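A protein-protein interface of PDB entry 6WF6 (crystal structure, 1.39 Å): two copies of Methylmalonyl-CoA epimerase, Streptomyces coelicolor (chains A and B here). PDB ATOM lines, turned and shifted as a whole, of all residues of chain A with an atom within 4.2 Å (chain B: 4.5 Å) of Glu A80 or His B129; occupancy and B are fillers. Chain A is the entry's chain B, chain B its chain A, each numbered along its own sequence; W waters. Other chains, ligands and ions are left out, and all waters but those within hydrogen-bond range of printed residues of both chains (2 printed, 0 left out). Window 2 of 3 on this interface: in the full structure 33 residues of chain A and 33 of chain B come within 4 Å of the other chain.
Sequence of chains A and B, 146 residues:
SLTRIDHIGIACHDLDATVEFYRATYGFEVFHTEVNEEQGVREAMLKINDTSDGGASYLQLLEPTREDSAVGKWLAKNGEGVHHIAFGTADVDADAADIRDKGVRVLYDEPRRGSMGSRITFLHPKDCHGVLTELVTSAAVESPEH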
ATOM      1  N   ALA A  11      -1.302 -14.690 -22.366  1.00  0.00           N
ATOM      2  CA  ALA A  11      -0.074 -15.299 -22.880  1.00  0.00           C
ATOM      3  C   ALA A  11       0.624 -14.314 -23.821  1.00  0.00           C
ATOM      4  O   ALA A  11      -0.023 -13.627 -24.620  1.00  0.00           O
ATOM      5  CB  ALA A  11      -0.454 -16.564 -23.598  1.00  0.00           C
ATOM      6  N   CYS A  12       1.954 -14.314 -23.749  1.00  0.00           N
ATOM      7  CA  CYS A  12       2.777 -13.414 -24.561  1.00  0.00           C
ATOM      8  C   CYS A  12       4.109 -14.083 -24.891  1.00  0.00           C
ATOM      9  O   CYS A  12       4.533 -14.999 -24.197  1.00  0.00           O
ATOM     10  CB  CYS A  12       2.928 -12.064 -23.891  1.00  0.00           C
ATOM     11  SG  CYS A  12       3.821 -12.154 -22.321  1.00  0.00           S
ATOM     12  N   HIS A  13       4.708 -13.598 -25.974  1.00  0.00           N
ATOM     13  CA  HIS A  13       5.989 -14.144 -26.471  1.00  0.00           C
ATOM     14  C   HIS A  13       7.152 -13.710 -25.596  1.00  0.00           C
ATOM     15  O   HIS A  13       8.077 -14.511 -25.383  1.00  0.00           O
ATOM     16  CB  HIS A  13       6.217 -13.672 -27.895  1.00  0.00           C
ATOM     17  CG  HIS A  13       5.252 -14.225 -28.882  1.00  0.00           C
ATOM     18  ND1 HIS A  13       5.039 -15.574 -29.018  1.00  0.00           N
ATOM     19  CD2 HIS A  13       4.520 -13.604 -29.821  1.00  0.00           C
ATOM     20  CE1 HIS A  13       4.160 -15.767 -29.980  1.00  0.00           C
ATOM     21  NE2 HIS A  13       3.813 -14.593 -30.458  1.00  0.00           N
ATOM     22  N   THR A  18       6.101  -7.240 -22.677  1.00  0.00           N
ATOM     23  CA  THR A  18       4.647  -7.131 -22.411  1.00  0.00           C
ATOM     24  C   THR A  18       4.438  -6.373 -21.109  1.00  0.00           C
ATOM     25  O   THR A  18       3.554  -5.500 -21.036  1.00  0.00           O
ATOM     26  CB  THR A  18       3.927  -8.461 -22.505  1.00  0.00           C
ATOM     27  OG1 THR A  18       4.220  -9.034 -23.791  1.00  0.00           O
ATOM     28  CG2 THR A  18       2.428  -8.265 -22.375  1.00  0.00           C
ATOM     29  N   PHE A  21       4.872  -2.753 -21.726  1.00  0.00           N
ATOM     30  CA  PHE A  21       3.666  -2.204 -22.382  1.00  0.00           C
ATOM     31  C   PHE A  21       2.616  -1.870 -21.312  1.00  0.00           C
ATOM     32  O   PHE A  21       2.020  -0.760 -21.325  1.00  0.00           O
ATOM     33  CB  PHE A  21       3.088  -3.173 -23.404  1.00  0.00           C
ATOM     34  CG  PHE A  21       1.685  -2.794 -23.826  1.00  0.00           C
ATOM     35  CD1 PHE A  21       1.449  -1.726 -24.667  1.00  0.00           C
ATOM     36  CD2 PHE A  21       0.604  -3.478 -23.311  1.00  0.00           C
ATOM     37  CE1 PHE A  21       0.145  -1.337 -24.991  1.00  0.00           C
ATOM     38  CE2 PHE A  21      -0.691  -3.082 -23.628  1.00  0.00           C
ATOM     39  CZ  PHE A  21      -0.902  -2.008 -24.444  1.00  0.00           C
ATOM     40  N   LEU A  75       0.332 -20.488 -27.799  1.00  0.00           N
ATOM     41  CA  LEU A  75       0.831 -19.306 -28.557  1.00  0.00           C
ATOM     42  C   LEU A  75       1.110 -19.615 -30.035  1.00  0.00           C
ATOM     43  O   LEU A  75       0.810 -18.773 -30.874  1.00  0.00           O
ATOM     44  CB  LEU A  75       2.095 -18.728 -27.922  1.00  0.00           C
ATOM     45  CG  LEU A  75       1.844 -17.866 -26.698  1.00  0.00           C
ATOM     46  CD1 LEU A  75       3.150 -17.658 -25.957  1.00  0.00           C
ATOM     47  CD2 LEU A  75       1.206 -16.522 -27.085  1.00  0.00           C
ATOM     48  N   GLY A  79      -1.534 -17.128 -31.336  1.00  0.00           N
ATOM     49  CA  GLY A  79      -0.869 -15.833 -31.130  1.00  0.00           C
ATOM     50  C   GLY A  79      -1.143 -15.283 -29.731  1.00  0.00           C
ATOM     51  O   GLY A  79      -1.812 -15.944 -28.948  1.00  0.00           O
ATOM     52  N   GLU A  80      -0.572 -14.130 -29.447  1.00  0.00           N
ATOM     53  CA  GLU A  80      -0.687 -13.501 -28.119  1.00  0.00           C
ATOM     54  C   GLU A  80      -2.140 -13.159 -27.792  1.00  0.00           C
ATOM     55  O   GLU A  80      -2.864 -12.700 -28.706  1.00  0.00           O
ATOM     56  CB  GLU A  80       0.142 -12.235 -28.059  1.00  0.00           C
ATOM     57  CG  GLU A  80       1.615 -12.466 -28.310  1.00  0.00           C
ATOM     58  CD  GLU A  80       2.449 -11.250 -27.948  1.00  0.00           C
ATOM     59  OE1 GLU A  80       2.209 -10.172 -28.541  1.00  0.00           O
ATOM     60  OE2 GLU A  80       3.366 -11.406 -27.153  1.00  0.00           O
ATOM     61  N   GLY A  81      -2.508 -13.231 -26.524  1.00  0.00           N
ATOM     62  CA  GLY A  81      -3.840 -12.770 -26.103  1.00  0.00           C
ATOM     63  C   GLY A  81      -4.299 -13.432 -24.842  1.00  0.00           C
ATOM     64  O   GLY A  81      -3.491 -14.052 -24.121  1.00  0.00           O
ATOM     65  N   PRO B 125      -6.585  -4.205 -30.578  1.00  0.00           N
ATOM     66  CA  PRO B 125      -5.867  -5.362 -30.001  1.00  0.00           C
ATOM     67  C   PRO B 125      -4.439  -5.507 -30.550  1.00  0.00           C
ATOM     68  O   PRO B 125      -3.567  -6.030 -29.856  1.00  0.00           O
ATOM     69  CB  PRO B 125      -6.759  -6.522 -30.358  1.00  0.00           C
ATOM     70  CG  PRO B 125      -7.561  -6.052 -31.547  1.00  0.00           C
ATOM     71  CD  PRO B 125      -7.811  -4.599 -31.260  1.00  0.00           C
ATOM     72  N   ASP B 127      -2.289  -3.217 -30.895  1.00  0.00           N
ATOM     73  CA  ASP B 127      -1.403  -2.366 -30.084  1.00  0.00           C
ATOM     74  C   ASP B 127      -1.340  -2.853 -28.632  1.00  0.00           C
ATOM     75  O   ASP B 127      -0.599  -2.241 -27.828  1.00  0.00           O
ATOM     76  CB  ASP B 127      -1.909  -0.924 -30.091  1.00  0.00           C
ATOM     77  CG  ASP B 127      -1.767  -0.267 -31.434  1.00  0.00           C
ATOM     78  OD1 ASP B 127      -0.858  -0.677 -32.206  1.00  0.00           O
ATOM     79  OD2 ASP B 127      -2.589   0.601 -31.734  1.00  0.00           O
ATOM     80  N   CYS B 128      -2.111  -3.880 -28.300  1.00  0.00           N
ATOM     81  CA  CYS B 128      -2.231  -4.385 -26.890  1.00  0.00           C
ATOM     82  C   CYS B 128      -1.855  -5.854 -26.825  1.00  0.00           C
ATOM     83  O   CYS B 128      -2.439  -6.604 -26.022  1.00  0.00           O
ATOM     84  CB  CYS B 128      -3.647  -4.186 -26.391  1.00  0.00           C
ATOM     85  SG  CYS B 128      -4.227  -2.466 -26.379  1.00  0.00           S
ATOM     86  N   HIS B 129      -0.908  -6.303 -27.608  1.00  0.00           N
ATOM     87  CA  HIS B 129      -0.409  -7.700 -27.571  1.00  0.00           C
ATOM     88  C   HIS B 129      -1.594  -8.672 -27.727  1.00  0.00           C
ATOM     89  O   HIS B 129      -1.650  -9.744 -27.076  1.00  0.00           O
ATOM     90  CB  HIS B 129       0.523  -7.947 -26.371  1.00  0.00           C
ATOM     91  CG  HIS B 129       1.799  -7.219 -26.481  1.00  0.00           C
ATOM     92  ND1 HIS B 129       2.843  -7.787 -27.183  1.00  0.00           N
ATOM     93  CD2 HIS B 129       2.207  -6.021 -26.017  1.00  0.00           C
ATOM     94  CE1 HIS B 129       3.859  -6.928 -27.132  1.00  0.00           C
ATOM     95  NE2 HIS B 129       3.514  -5.860 -26.429  1.00  0.00           N
ATOM     96  N   GLY B 130      -2.527  -8.395 -28.652  1.00  0.00           N
ATOM     97  CA  GLY B 130      -3.602  -9.306 -28.990  1.00  0.00           C
ATOM     98  C   GLY B 130      -4.860  -9.162 -28.146  1.00  0.00           C
ATOM     99  O   GLY B 130      -5.744  -9.993 -28.303  1.00  0.00           O
ATOM    100  N   VAL B 131      -4.886  -8.261 -27.166  1.00  0.00           N
ATOM    101  CA  VAL B 131      -6.035  -8.159 -26.241  1.00  0.00           C
ATOM    102  C   VAL B 131      -6.878  -6.937 -26.586  1.00  0.00           C
ATOM    103  O   VAL B 131      -6.425  -5.819 -26.410  1.00  0.00           O
ATOM    104  CB  VAL B 131      -5.552  -8.115 -24.798  1.00  0.00           C
ATOM    105  CG1 VAL B 131      -6.702  -8.013 -23.832  1.00  0.00           C
ATOM    106  CG2 VAL B 131      -4.728  -9.333 -24.423  1.00  0.00           C
HETATM  107  O   HOH W   1      -0.653 -10.622 -24.688  1.00  0.00           O
HETATM  108  O   HOH W   2      -5.913 -12.525 -29.349  1.00  0.00           O
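No position is printed for both chains.
Among the printed residues, merely in contact across the chains: Phe A21 with Asp B127 (3.1 Å), Glu A80 with Gly B130 (3.5 Å), Gly A81 with His B129 (3.6 Å), Phe A21 with Cys B128 (3.7 Å), Thr A18 with His B129 (3.9 Å), Gly A81 with Val B131 (3.9 Å) and Phe A21 with His B129 (3.9 Å).
A ring nitrogen (ND1) of His B129 sits at hydrogen-bond distance from the side-chain carboxylate of Glu A80, 2.8 Å away.
The backbone carbonyl oxygen (O) of Pro B125 lies within hydrogen-bond range of the backbone NH (N) of Gly B130 (2.9 Å).
The backbone carbonyl oxygen (O) of Gly A81 lies within hydrogen-bond range of the backbone NH (N) of Ala A11.
SG of Cys A12 sits close to OG1 of Thr A18 (3.5 Å).
OE2 of Glu A80 lies within hydrogen-bond range of N of His A13 (2.8 Å).
Of chain B, only His B129 (2.8 Å) and Gly B130 (3.5 Å) come within 4 Å of Glu A80.
Printed residues of chain A within 4 Å of His B129: Thr A18 (3.9 Å), Phe A21 (3.9 Å), Glu A80 (2.8 Å) and Gly A81 (3.6 Å).
Printed residues of chain B within 4 Å of Thr A18: His B129.
Of the printed residues of chain A, Gly B130 touches Glu A80.
Pro B125 touches none of the printed residues of chain A.
The nearest printed residue of chain A that does not touch His B129 is Ala A11 (4.9 Å).
Printed residues of chain A that touch a printed residue of chain B: Thr A18, Phe A21, Glu A80 and Gly A81.
Hydrophobic or aromatic side chains of chain A within 4 Å of the printed part of chain B: Phe A21.
Of the 6 printed residues of chain B, 5 touch a printed residue of chain A.
Hydrophobic or aromatic side chains of chain B that line the printed part of chain A: His B129 and Val B131.
Among the printed residues, 8 pairs touch across the chains.
Water W1 bridges O of His B129 and O of Ala A11.
Water W2 lies within hydrogen-bond range of O of Gly B130 (2.7 Å) and O of Glu A80 (3.1 Å).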
